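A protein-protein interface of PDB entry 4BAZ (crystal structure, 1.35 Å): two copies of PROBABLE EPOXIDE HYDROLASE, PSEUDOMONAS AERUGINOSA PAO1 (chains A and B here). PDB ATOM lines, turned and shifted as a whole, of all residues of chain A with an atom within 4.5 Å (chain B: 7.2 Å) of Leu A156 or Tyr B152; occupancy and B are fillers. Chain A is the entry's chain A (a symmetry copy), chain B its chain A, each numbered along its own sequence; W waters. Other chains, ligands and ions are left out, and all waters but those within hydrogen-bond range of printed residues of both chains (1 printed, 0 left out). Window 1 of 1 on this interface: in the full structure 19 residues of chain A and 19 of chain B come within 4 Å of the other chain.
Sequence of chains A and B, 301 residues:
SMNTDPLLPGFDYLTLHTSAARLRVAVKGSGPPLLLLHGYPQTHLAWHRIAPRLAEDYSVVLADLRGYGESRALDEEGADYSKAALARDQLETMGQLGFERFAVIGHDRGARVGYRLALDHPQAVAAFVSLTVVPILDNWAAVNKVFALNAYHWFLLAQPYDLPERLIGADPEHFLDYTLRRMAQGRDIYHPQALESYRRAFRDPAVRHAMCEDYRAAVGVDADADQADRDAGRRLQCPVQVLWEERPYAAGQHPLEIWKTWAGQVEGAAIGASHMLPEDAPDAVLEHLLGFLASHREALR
NH2 of Arg B182 lies within hydrogen-bond range of O of Leu B149, at 3.4 Å. The guanidinium group (NH2) of Arg B182 is in hydrogen-bond range of the backbone carbonyl oxygen (O) of Asn B150, at 3.0 Å. The guanidinium group (NH1) of Arg B182 is in hydrogen-bond range of the side-chain hydroxyl (OH) of Tyr B178, at 2.9 Å. The backbone carbonyl oxygen (O) of Phe A155 is in hydrogen-bond range of the side-chain amide nitrogen (NE2) of Gln A159 (2.9 Å).
Tyr A152 touches Leu B156, and with the chains exchanged Leu A156 touches Tyr B152. Tyr A152 touches Leu B163, and with the chains exchanged Leu A163 touches Tyr B152. Leu A167 touches its own counterpart, Leu B167.
Water W1 lies within hydrogen-bond range of the backbone carbonyl oxygen (O) of Tyr B152 and the backbone carbonyl oxygen (O) of Tyr A152.
Of chain B, only Tyr B152 comes within 4 Å of Leu A156. Printed residues of chain A within 4 Å of Tyr B152: Leu A156 (3.9 Å), Gln A159 (3.4 Å) and Leu A163 (3.7 Å). Of the printed residues of chain B, Leu A167 touches Leu B167. Of the printed residues of chain A, Leu B156 touches Tyr A152 (3.9 Å). His B153 touches none of the printed residues of chain A. The nearest printed residue of chain A that does not touch Leu B167 is Leu A156 (4.2 Å).
CE2 of Tyr A152 touches CD1 of Leu B156, at 3.9 Å. Leu B163 touches Tyr A152. Ala B148 touches Phe A155 (CB to CE1, 3.5 Å). Phe A155 touches Leu B149. CE2 of Tyr B152 touches CD1 of Leu A156 (3.9 Å). Gln A159 touches Tyr B152 (CD to CD1, 3.4 Å). Leu A163 touches Tyr B152 (CD1 to OH, 3.7 Å). Leu A163 touches Tyr B178 (CD2 to CD2, 3.7 Å). Leu A167 touches Leu B167 (O to CD2, 3.4 Å).
Hydrophobic or aromatic side chains of chain A within 4 Å of the printed part of chain B: Tyr A152, Phe A155, Leu A156, Leu A163 and Leu A167. Of the 21 printed residues of chain B, 8 touch a printed residue of chain A. Hydrophobic or aromatic side chains of chain B that line the printed part of chain A: Ala B148, Leu B149, Tyr B152, Leu B156, Leu B163, Leu B167 and Tyr B178. Along chain B the printed residues that touch a printed residue of chain A span positions 148 to 182. Among the printed residues, no Asp or Glu carboxylate lies within 4 Å of a Lys or Arg side-chain nitrogen of the other chain.
O of Leu B149 is in hydrogen-bond range of NE2 of Gln A159, 2.9 Å away. NH1 of Arg B182 sits at hydrogen-bond distance from OE1 of Gln A159 (2.8 Å).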
ATOM      1  N   TYR A 152     -10.705   3.564   6.811  1.00  0.00           N
ATOM      2  CA  TYR A 152     -11.122   3.126   5.485  1.00  0.00           C
ATOM      3  C   TYR A 152     -12.634   3.195   5.330  1.00  0.00           C
ATOM      4  O   TYR A 152     -13.140   3.412   4.220  1.00  0.00           O
ATOM      5  CB  TYR A 152     -10.603   1.717   5.146  1.00  0.00           C
ATOM      6  CG  TYR A 152     -11.412   0.656   5.811  1.00  0.00           C
ATOM      7  CD1 TYR A 152     -11.234   0.340   7.162  1.00  0.00           C
ATOM      8  CD2 TYR A 152     -12.420  -0.006   5.116  1.00  0.00           C
ATOM      9  CE1 TYR A 152     -12.075  -0.578   7.804  1.00  0.00           C
ATOM     10  CE2 TYR A 152     -13.273  -0.893   5.762  1.00  0.00           C
ATOM     11  CZ  TYR A 152     -13.112  -1.168   7.104  1.00  0.00           C
ATOM     12  OH  TYR A 152     -13.996  -2.041   7.726  1.00  0.00           O
ATOM     13  N   HIS A 153     -13.344   2.951   6.441  1.00  0.00           N
ATOM     14  CA  HIS A 153     -14.793   2.914   6.396  1.00  0.00           C
ATOM     15  C   HIS A 153     -15.415   4.270   6.088  1.00  0.00           C
ATOM     16  O   HIS A 153     -16.550   4.336   5.596  1.00  0.00           O
ATOM     17  CB  HIS A 153     -15.340   2.294   7.683  1.00  0.00           C
ATOM     18  CG  HIS A 153     -15.047   3.090   8.902  1.00  0.00           C
ATOM     19  ND1 HIS A 153     -13.778   3.285   9.351  1.00  0.00           N
ATOM     20  CD2 HIS A 153     -15.855   3.761   9.749  1.00  0.00           C
ATOM     21  CE1 HIS A 153     -13.790   4.039  10.415  1.00  0.00           C
ATOM     22  NE2 HIS A 153     -15.048   4.334  10.697  1.00  0.00           N
ATOM     23  N   TRP A 154     -14.699   5.352   6.375  1.00  0.00           N
ATOM     24  CA  TRP A 154     -15.219   6.666   6.006  1.00  0.00           C
ATOM     25  C   TRP A 154     -15.419   6.804   4.506  1.00  0.00           C
ATOM     26  O   TRP A 154     -16.267   7.534   4.019  1.00  0.00           O
ATOM     27  CB  TRP A 154     -14.287   7.766   6.476  1.00  0.00           C
ATOM     28  CG  TRP A 154     -14.266   8.021   7.942  1.00  0.00           C
ATOM     29  CD1 TRP A 154     -14.475   7.128   8.960  1.00  0.00           C
ATOM     30  CD2 TRP A 154     -14.071   9.306   8.573  1.00  0.00           C
ATOM     31  NE1 TRP A 154     -14.423   7.786  10.179  1.00  0.00           N
ATOM     32  CE2 TRP A 154     -14.179   9.117   9.966  1.00  0.00           C
ATOM     33  CE3 TRP A 154     -13.840  10.587   8.086  1.00  0.00           C
ATOM     34  CZ2 TRP A 154     -14.056  10.182  10.880  1.00  0.00           C
ATOM     35  CZ3 TRP A 154     -13.719  11.631   8.991  1.00  0.00           C
ATOM     36  CH2 TRP A 154     -13.840  11.423  10.362  1.00  0.00           C
ATOM     37  N   PHE A 155     -14.592   6.065   3.767  1.00  0.00           N
ATOM     38  CA  PHE A 155     -14.590   6.111   2.314  1.00  0.00           C
ATOM     39  C   PHE A 155     -15.482   5.006   1.768  1.00  0.00           C
ATOM     40  O   PHE A 155     -16.241   5.237   0.816  1.00  0.00           O
ATOM     41  CB  PHE A 155     -13.142   6.038   1.793  1.00  0.00           C
ATOM     42  CG  PHE A 155     -12.326   7.173   2.350  1.00  0.00           C
ATOM     43  CD1 PHE A 155     -12.469   8.448   1.837  1.00  0.00           C
ATOM     44  CD2 PHE A 155     -11.530   7.017   3.456  1.00  0.00           C
ATOM     45  CE1 PHE A 155     -11.820   9.517   2.410  1.00  0.00           C
ATOM     46  CE2 PHE A 155     -10.888   8.073   4.042  1.00  0.00           C
ATOM     47  CZ  PHE A 155     -11.021   9.340   3.509  1.00  0.00           C
ATOM     48  N   LEU A 156     -15.452   3.802   2.375  1.00  0.00           N
ATOM     49  CA  LEU A 156     -16.361   2.735   1.929  1.00  0.00           C
ATOM     50  C   LEU A 156     -17.836   3.119   2.109  1.00  0.00           C
ATOM     51  O   LEU A 156     -18.653   2.966   1.208  1.00  0.00           O
ATOM     52  CB  LEU A 156     -16.086   1.438   2.716  1.00  0.00           C
ATOM     53  CG  LEU A 156     -17.096   0.314   2.540  1.00  0.00           C
ATOM     54  CD1 LEU A 156     -17.192  -0.159   1.113  1.00  0.00           C
ATOM     55  CD2 LEU A 156     -16.759  -0.816   3.493  1.00  0.00           C
ATOM     56  N   LEU A 157     -18.195   3.564   3.329  1.00  0.00           N
ATOM     57  CA  LEU A 157     -19.590   3.773   3.686  1.00  0.00           C
ATOM     58  C   LEU A 157     -20.192   4.977   2.951  1.00  0.00           C
ATOM     59  O   LEU A 157     -21.404   5.088   2.828  1.00  0.00           O
ATOM     60  CB  LEU A 157     -19.749   3.913   5.196  1.00  0.00           C
ATOM     61  CG  LEU A 157     -19.322   2.713   6.047  1.00  0.00           C
ATOM     62  CD1 LEU A 157     -19.449   3.057   7.524  1.00  0.00           C
ATOM     63  CD2 LEU A 157     -20.026   1.452   5.629  1.00  0.00           C
ATOM     64  N   ALA A 158     -19.328   5.827   2.407  1.00  0.00           N
ATOM     65  CA  ALA A 158     -19.726   6.978   1.611  1.00  0.00           C
ATOM     66  C   ALA A 158     -19.926   6.688   0.110  1.00  0.00           C
ATOM     67  O   ALA A 158     -20.291   7.593  -0.663  1.00  0.00           O
ATOM     68  CB  ALA A 158     -18.765   8.153   1.807  1.00  0.00           C
ATOM     69  N   GLN A 159     -19.605   5.473  -0.326  1.00  0.00           N
ATOM     70  CA  GLN A 159     -19.795   5.136  -1.741  1.00  0.00           C
ATOM     71  C   GLN A 159     -21.276   5.157  -2.114  1.00  0.00           C
ATOM     72  O   GLN A 159     -22.126   5.067  -1.227  1.00  0.00           O
ATOM     73  CB  GLN A 159     -19.149   3.798  -2.049  1.00  0.00           C
ATOM     74  CG  GLN A 159     -17.641   3.795  -1.850  1.00  0.00           C
ATOM     75  CD  GLN A 159     -16.951   4.860  -2.685  1.00  0.00           C
ATOM     76  OE1 GLN A 159     -17.162   4.952  -3.901  1.00  0.00           O
ATOM     77  NE2 GLN A 159     -16.160   5.685  -2.030  1.00  0.00           N
ATOM     78  N   LEU A 163     -23.817   0.192  -2.754  1.00  0.00           N
ATOM     79  CA  LEU A 163     -22.563  -0.553  -2.688  1.00  0.00           C
ATOM     80  C   LEU A 163     -22.208  -0.949  -1.241  1.00  0.00           C
ATOM     81  O   LEU A 163     -22.049  -2.141  -0.939  1.00  0.00           O
ATOM     82  CB  LEU A 163     -21.442   0.247  -3.399  1.00  0.00           C
ATOM     83  CG  LEU A 163     -20.046  -0.402  -3.553  1.00  0.00           C
ATOM     84  CD1 LEU A 163     -19.211  -0.354  -2.266  1.00  0.00           C
ATOM     85  CD2 LEU A 163     -20.199  -1.800  -4.123  1.00  0.00           C
ATOM     86  N   PRO A 164     -22.045   0.044  -0.323  1.00  0.00           N
ATOM     87  CA  PRO A 164     -21.638  -0.394   0.997  1.00  0.00           C
ATOM     88  C   PRO A 164     -22.717  -1.203   1.711  1.00  0.00           C
ATOM     89  O   PRO A 164     -22.388  -2.137   2.462  1.00  0.00           O
ATOM     90  CB  PRO A 164     -21.286   0.915   1.730  1.00  0.00           C
ATOM     91  CG  PRO A 164     -22.094   1.962   1.019  1.00  0.00           C
ATOM     92  CD  PRO A 164     -22.087   1.515  -0.446  1.00  0.00           C
ATOM     93  N   LEU A 167     -22.223  -4.746   0.827  1.00  0.00           N
ATOM     94  CA  LEU A 167     -21.048  -5.372   1.418  1.00  0.00           C
ATOM     95  C   LEU A 167     -21.193  -5.619   2.921  1.00  0.00           C
ATOM     96  O   LEU A 167     -20.874  -6.701   3.411  1.00  0.00           O
ATOM     97  CB  LEU A 167     -19.804  -4.564   1.125  1.00  0.00           C
ATOM     98  CG  LEU A 167     -19.398  -4.400  -0.319  1.00  0.00           C
ATOM     99  CD1 LEU A 167     -18.036  -3.694  -0.424  1.00  0.00           C
ATOM    100  CD2 LEU A 167     -19.377  -5.682  -1.085  1.00  0.00           C
ATOM    101  N   TYR B  40      -6.342  -5.353 -12.533  1.00  0.00           N
ATOM    102  CA  TYR B  40      -7.444  -5.729 -11.678  1.00  0.00           C
ATOM    103  C   TYR B  40      -8.767  -5.199 -12.223  1.00  0.00           C
ATOM    104  O   TYR B  40      -8.801  -4.077 -12.749  1.00  0.00           O
ATOM    105  CB  TYR B  40      -7.216  -5.081 -10.297  1.00  0.00           C
ATOM    106  CG  TYR B  40      -8.421  -5.025  -9.385  1.00  0.00           C
ATOM    107  CD1 TYR B  40      -9.258  -3.928  -9.383  1.00  0.00           C
ATOM    108  CD2 TYR B  40      -8.673  -6.029  -8.469  1.00  0.00           C
ATOM    109  CE1 TYR B  40     -10.305  -3.826  -8.482  1.00  0.00           C
ATOM    110  CE2 TYR B  40      -9.761  -5.962  -7.623  1.00  0.00           C
ATOM    111  CZ  TYR B  40     -10.548  -4.845  -7.604  1.00  0.00           C
ATOM    112  OH  TYR B  40     -11.615  -4.784  -6.724  1.00  0.00           O
ATOM    113  N   VAL B 146     -10.558  13.302  -2.129  1.00  0.00           N
ATOM    114  CA  VAL B 146     -11.169  12.812  -3.360  1.00  0.00           C
ATOM    115  C   VAL B 146     -10.455  11.572  -3.870  1.00  0.00           C
ATOM    116  O   VAL B 146     -11.109  10.681  -4.408  1.00  0.00           O
ATOM    117  CB  VAL B 146     -11.238  13.954  -4.409  1.00  0.00           C
ATOM    118  CG1 VAL B 146     -11.548  13.396  -5.783  1.00  0.00           C
ATOM    119  CG2 VAL B 146     -12.331  14.921  -3.960  1.00  0.00           C
ATOM    120  N   PHE B 147      -9.148  11.474  -3.717  1.00  0.00           N
ATOM    121  CA  PHE B 147      -8.411  10.248  -4.067  1.00  0.00           C
ATOM    122  C   PHE B 147      -9.031   9.054  -3.359  1.00  0.00           C
ATOM    123  O   PHE B 147      -9.318   8.003  -3.947  1.00  0.00           O
ATOM    124  CB  PHE B 147      -6.942  10.383  -3.627  1.00  0.00           C
ATOM    125  CG  PHE B 147      -6.056   9.200  -4.016  1.00  0.00           C
ATOM    126  CD1 PHE B 147      -6.183   7.966  -3.402  1.00  0.00           C
ATOM    127  CD2 PHE B 147      -5.086   9.351  -4.993  1.00  0.00           C
ATOM    128  CE1 PHE B 147      -5.359   6.893  -3.738  1.00  0.00           C
ATOM    129  CE2 PHE B 147      -4.274   8.271  -5.329  1.00  0.00           C
ATOM    130  CZ  PHE B 147      -4.415   7.061  -4.699  1.00  0.00           C
ATOM    131  N   ALA B 148      -9.192   9.200  -2.059  1.00  0.00           N
ATOM    132  CA  ALA B 148      -9.641   8.102  -1.208  1.00  0.00           C
ATOM    133  C   ALA B 148     -11.097   7.726  -1.489  1.00  0.00           C
ATOM    134  O   ALA B 148     -11.482   6.556  -1.338  1.00  0.00           O
ATOM    135  CB  ALA B 148      -9.355   8.383   0.239  1.00  0.00           C
ATOM    136  N   LEU B 149     -11.929   8.702  -1.854  1.00  0.00           N
ATOM    137  CA  LEU B 149     -13.288   8.389  -2.283  1.00  0.00           C
ATOM    138  C   LEU B 149     -13.314   7.652  -3.612  1.00  0.00           C
ATOM    139  O   LEU B 149     -14.031   6.662  -3.766  1.00  0.00           O
ATOM    140  CB  LEU B 149     -14.148   9.639  -2.295  1.00  0.00           C
ATOM    141  CG  LEU B 149     -14.466  10.268  -0.971  1.00  0.00           C
ATOM    142  CD1 LEU B 149     -14.968  11.696  -1.112  1.00  0.00           C
ATOM    143  CD2 LEU B 149     -15.499   9.399  -0.223  1.00  0.00           C
ATOM    144  N   ASN B 150     -12.544   8.136  -4.570  1.00  0.00           N
ATOM    145  CA  ASN B 150     -12.597   7.552  -5.905  1.00  0.00           C
ATOM    146  C   ASN B 150     -11.988   6.151  -5.903  1.00  0.00           C
ATOM    147  O   ASN B 150     -12.462   5.268  -6.586  1.00  0.00           O
ATOM    148  CB  ASN B 150     -11.852   8.456  -6.914  1.00  0.00           C
ATOM    149  CG  ASN B 150     -12.617   9.719  -7.257  1.00  0.00           C
ATOM    150  OD1 ASN B 150     -13.808   9.818  -6.983  1.00  0.00           O
ATOM    151  ND2 ASN B 150     -11.935  10.697  -7.865  1.00  0.00           N
ATOM    152  N   ALA B 151     -10.885   6.007  -5.168  1.00  0.00           N
ATOM    153  CA  ALA B 151     -10.110   4.769  -5.060  1.00  0.00           C
ATOM    154  C   ALA B 151     -10.297   4.109  -3.682  1.00  0.00           C
ATOM    155  O   ALA B 151      -9.352   3.574  -3.088  1.00  0.00           O
ATOM    156  CB  ALA B 151      -8.649   5.007  -5.401  1.00  0.00           C
ATOM    157  N   TYR B 152     -11.555   4.077  -3.205  1.00  0.00           N
ATOM    158  CA  TYR B 152     -11.838   3.570  -1.868  1.00  0.00           C
ATOM    159  C   TYR B 152     -11.329   2.146  -1.697  1.00  0.00           C
ATOM    160  O   TYR B 152     -10.962   1.743  -0.585  1.00  0.00           O
ATOM    161  CB  TYR B 152     -13.333   3.661  -1.514  1.00  0.00           C
ATOM    162  CG  TYR B 152     -14.119   2.568  -2.153  1.00  0.00           C
ATOM    163  CD1 TYR B 152     -14.489   2.626  -3.501  1.00  0.00           C
ATOM    164  CD2 TYR B 152     -14.451   1.422  -1.437  1.00  0.00           C
ATOM    165  CE1 TYR B 152     -15.129   1.545  -4.120  1.00  0.00           C
ATOM    166  CE2 TYR B 152     -15.058   0.337  -2.060  1.00  0.00           C
ATOM    167  CZ  TYR B 152     -15.383   0.392  -3.399  1.00  0.00           C
ATOM    168  OH  TYR B 152     -15.967  -0.718  -3.998  1.00  0.00           O
ATOM    169  N   HIS B 153     -11.368   1.380  -2.796  1.00  0.00           N
ATOM    170  CA  HIS B 153     -10.981  -0.017  -2.734  1.00  0.00           C
ATOM    171  C   HIS B 153      -9.498  -0.211  -2.440  1.00  0.00           C
ATOM    172  O   HIS B 153      -9.100  -1.271  -1.937  1.00  0.00           O
ATOM    173  CB  HIS B 153     -11.429  -0.740  -4.005  1.00  0.00           C
ATOM    174  CG  HIS B 153     -10.766  -0.246  -5.240  1.00  0.00           C
ATOM    175  ND1 HIS B 153     -10.954   1.018  -5.706  1.00  0.00           N
ATOM    176  CD2 HIS B 153      -9.899  -0.837  -6.088  1.00  0.00           C
ATOM    177  CE1 HIS B 153     -10.241   1.210  -6.781  1.00  0.00           C
ATOM    178  NE2 HIS B 153      -9.596   0.088  -7.053  1.00  0.00           N
ATOM    179  N   TRP B 154      -8.676   0.783  -2.751  1.00  0.00           N
ATOM    180  CA  TRP B 154      -7.263   0.675  -2.397  1.00  0.00           C
ATOM    181  C   TRP B 154      -7.056   0.546  -0.897  1.00  0.00           C
ATOM    182  O   TRP B 154      -6.105  -0.044  -0.411  1.00  0.00           O
ATOM    183  CB  TRP B 154      -6.488   1.880  -2.893  1.00  0.00           C
ATOM    184  CG  TRP B 154      -6.267   1.952  -4.363  1.00  0.00           C
ATOM    185  CD1 TRP B 154      -7.071   1.476  -5.365  1.00  0.00           C
ATOM    186  CD2 TRP B 154      -5.102   2.504  -5.015  1.00  0.00           C
ATOM    187  NE1 TRP B 154      -6.471   1.700  -6.594  1.00  0.00           N
ATOM    188  CE2 TRP B 154      -5.266   2.324  -6.404  1.00  0.00           C
ATOM    189  CE3 TRP B 154      -3.938   3.105  -4.551  1.00  0.00           C
ATOM    190  CZ2 TRP B 154      -4.294   2.738  -7.335  1.00  0.00           C
ATOM    191  CZ3 TRP B 154      -2.985   3.511  -5.472  1.00  0.00           C
ATOM    192  CH2 TRP B 154      -3.164   3.314  -6.838  1.00  0.00           C
ATOM    193  N   PHE B 155      -7.995   1.134  -0.155  1.00  0.00           N
ATOM    194  CA  PHE B 155      -7.936   1.171   1.297  1.00  0.00           C
ATOM    195  C   PHE B 155      -8.727   0.004   1.870  1.00  0.00           C
ATOM    196  O   PHE B 155      -8.274  -0.640   2.826  1.00  0.00           O
ATOM    197  CB  PHE B 155      -8.422   2.542   1.803  1.00  0.00           C
ATOM    198  CG  PHE B 155      -7.580   3.645   1.219  1.00  0.00           C
ATOM    199  CD1 PHE B 155      -6.314   3.887   1.715  1.00  0.00           C
ATOM    200  CD2 PHE B 155      -7.975   4.345   0.107  1.00  0.00           C
ATOM    201  CE1 PHE B 155      -5.487   4.811   1.118  1.00  0.00           C
ATOM    202  CE2 PHE B 155      -7.158   5.257  -0.502  1.00  0.00           C
ATOM    203  CZ  PHE B 155      -5.902   5.507   0.014  1.00  0.00           C
ATOM    204  N   LEU B 156      -9.894  -0.328   1.280  1.00  0.00           N
ATOM    205  CA  LEU B 156     -10.644  -1.501   1.752  1.00  0.00           C
ATOM    206  C   LEU B 156      -9.849  -2.803   1.583  1.00  0.00           C
ATOM    207  O   LEU B 156      -9.747  -3.615   2.496  1.00  0.00           O
ATOM    208  CB  LEU B 156     -11.974  -1.628   0.982  1.00  0.00           C
ATOM    209  CG  LEU B 156     -12.753  -2.919   1.186  1.00  0.00           C
ATOM    210  CD1 LEU B 156     -13.161  -3.127   2.621  1.00  0.00           C
ATOM    211  CD2 LEU B 156     -13.942  -2.940   0.246  1.00  0.00           C
ATOM    212  N   LEU B 157      -9.333  -3.034   0.361  1.00  0.00           N
ATOM    213  CA  LEU B 157      -8.730  -4.313   0.016  1.00  0.00           C
ATOM    214  C   LEU B 157      -7.395  -4.528   0.740  1.00  0.00           C
ATOM    215  O   LEU B 157      -6.934  -5.652   0.875  1.00  0.00           O
ATOM    216  CB  LEU B 157      -8.567  -4.448  -1.494  1.00  0.00           C
ATOM    217  CG  LEU B 157      -9.849  -4.402  -2.331  1.00  0.00           C
ATOM    218  CD1 LEU B 157      -9.499  -4.446  -3.812  1.00  0.00           C
ATOM    219  CD2 LEU B 157     -10.845  -5.437  -1.887  1.00  0.00           C
ATOM    220  N   ALA B 158      -6.827  -3.445   1.261  1.00  0.00           N
ATOM    221  CA  ALA B 158      -5.601  -3.479   2.044  1.00  0.00           C
ATOM    222  C   ALA B 158      -5.804  -3.731   3.551  1.00  0.00           C
ATOM    223  O   ALA B 158      -4.823  -3.805   4.314  1.00  0.00           O
ATOM    224  CB  ALA B 158      -4.760  -2.220   1.819  1.00  0.00           C
ATOM    225  N   LEU B 163     -10.851  -9.303   6.556  1.00  0.00           N
ATOM    226  CA  LEU B 163     -11.930  -8.321   6.488  1.00  0.00           C
ATOM    227  C   LEU B 163     -12.428  -8.120   5.043  1.00  0.00           C
ATOM    228  O   LEU B 163     -13.618  -8.319   4.757  1.00  0.00           O
ATOM    229  CB  LEU B 163     -11.483  -7.005   7.174  1.00  0.00           C
ATOM    230  CG  LEU B 163     -12.509  -5.857   7.322  1.00  0.00           C
ATOM    231  CD1 LEU B 163     -12.721  -5.064   6.025  1.00  0.00           C
ATOM    232  CD2 LEU B 163     -13.795  -6.402   7.915  1.00  0.00           C
ATOM    233  N   LEU B 167     -16.079  -9.271   3.033  1.00  0.00           N
ATOM    234  CA  LEU B 167     -17.027  -8.338   2.438  1.00  0.00           C
ATOM    235  C   LEU B 167     -17.237  -8.572   0.941  1.00  0.00           C
ATOM    236  O   LEU B 167     -18.370  -8.590   0.464  1.00  0.00           O
ATOM    237  CB  LEU B 167     -16.613  -6.909   2.705  1.00  0.00           C
ATOM    238  CG  LEU B 167     -16.559  -6.451   4.142  1.00  0.00           C
ATOM    239  CD1 LEU B 167     -16.279  -4.941   4.221  1.00  0.00           C
ATOM    240  CD2 LEU B 167     -17.782  -6.793   4.927  1.00  0.00           C
ATOM    241  N   ILE B 168     -16.154  -8.733   0.180  1.00  0.00           N
ATOM    242  CA  ILE B 168     -16.281  -8.916  -1.265  1.00  0.00           C
ATOM    243  C   ILE B 168     -16.701 -10.326  -1.656  1.00  0.00           C
ATOM    244  O   ILE B 168     -17.174 -10.538  -2.765  1.00  0.00           O
ATOM    245  CB  ILE B 168     -15.005  -8.463  -2.023  1.00  0.00           C
ATOM    246  CG1 ILE B 168     -13.825  -9.427  -1.790  1.00  0.00           C
ATOM    247  CG2 ILE B 168     -14.645  -6.994  -1.715  1.00  0.00           C
ATOM    248  CD1 ILE B 168     -12.550  -9.062  -2.558  1.00  0.00           C
ATOM    249  N   PHE B 175     -20.096  -7.570  -6.888  1.00  0.00           N
ATOM    250  CA  PHE B 175     -19.010  -6.656  -6.676  1.00  0.00           C
ATOM    251  C   PHE B 175     -18.161  -6.546  -7.940  1.00  0.00           C
ATOM    252  O   PHE B 175     -17.704  -5.454  -8.303  1.00  0.00           O
ATOM    253  CB  PHE B 175     -18.156  -7.106  -5.494  1.00  0.00           C
ATOM    254  CG  PHE B 175     -17.047  -6.154  -5.169  1.00  0.00           C
ATOM    255  CD1 PHE B 175     -17.293  -4.986  -4.496  1.00  0.00           C
ATOM    256  CD2 PHE B 175     -15.764  -6.384  -5.603  1.00  0.00           C
ATOM    257  CE1 PHE B 175     -16.274  -4.112  -4.205  1.00  0.00           C
ATOM    258  CE2 PHE B 175     -14.719  -5.482  -5.342  1.00  0.00           C
ATOM    259  CZ  PHE B 175     -14.997  -4.334  -4.655  1.00  0.00           C
ATOM    260  N   TYR B 178     -20.103  -4.510 -10.605  1.00  0.00           N
ATOM    261  CA  TYR B 178     -20.118  -3.098 -10.216  1.00  0.00           C
ATOM    262  C   TYR B 178     -18.770  -2.449 -10.493  1.00  0.00           C
ATOM    263  O   TYR B 178     -18.676  -1.348 -11.052  1.00  0.00           O
ATOM    264  CB  TYR B 178     -20.470  -2.980  -8.726  1.00  0.00           C
ATOM    265  CG  TYR B 178     -20.304  -1.578  -8.208  1.00  0.00           C
ATOM    266  CD1 TYR B 178     -21.306  -0.643  -8.360  1.00  0.00           C
ATOM    267  CD2 TYR B 178     -19.140  -1.164  -7.615  1.00  0.00           C
ATOM    268  CE1 TYR B 178     -21.152   0.654  -7.923  1.00  0.00           C
ATOM    269  CE2 TYR B 178     -18.954   0.138  -7.198  1.00  0.00           C
ATOM    270  CZ  TYR B 178     -19.961   1.035  -7.346  1.00  0.00           C
ATOM    271  OH  TYR B 178     -19.812   2.332  -6.930  1.00  0.00           O
ATOM    272  N   THR B 179     -17.707  -3.134 -10.114  1.00  0.00           N
ATOM    273  CA  THR B 179     -16.360  -2.614 -10.272  1.00  0.00           C
ATOM    274  C   THR B 179     -15.998  -2.431 -11.740  1.00  0.00           C
ATOM    275  O   THR B 179     -15.458  -1.389 -12.123  1.00  0.00           O
ATOM    276  CB  THR B 179     -15.359  -3.562  -9.567  1.00  0.00           C
ATOM    277  OG1 THR B 179     -15.620  -3.534  -8.151  1.00  0.00           O
ATOM    278  CG2 THR B 179     -13.924  -3.183  -9.849  1.00  0.00           C
ATOM    279  N   ARG B 182     -17.877   0.555 -13.104  1.00  0.00           N
ATOM    280  CA  ARG B 182     -17.318   1.804 -12.590  1.00  0.00           C
ATOM    281  C   ARG B 182     -16.008   2.173 -13.294  1.00  0.00           C
ATOM    282  O   ARG B 182     -15.782   3.322 -13.695  1.00  0.00           O
ATOM    283  CB  ARG B 182     -17.164   1.682 -11.099  1.00  0.00           C
ATOM    284  CG  ARG B 182     -16.563   2.884 -10.433  1.00  0.00           C
ATOM    285  CD  ARG B 182     -16.763   2.795  -8.953  1.00  0.00           C
ATOM    286  NE  ARG B 182     -16.015   3.797  -8.223  1.00  0.00           N
ATOM    287  CZ  ARG B 182     -16.232   4.153  -6.979  1.00  0.00           C
ATOM    288  NH1 ARG B 182     -17.296   3.672  -6.349  1.00  0.00           N
ATOM    289  NH2 ARG B 182     -15.420   5.029  -6.374  1.00  0.00           N
HETATM  290  O   HOH W   1     -12.631   1.794   1.827  1.00  0.00           O
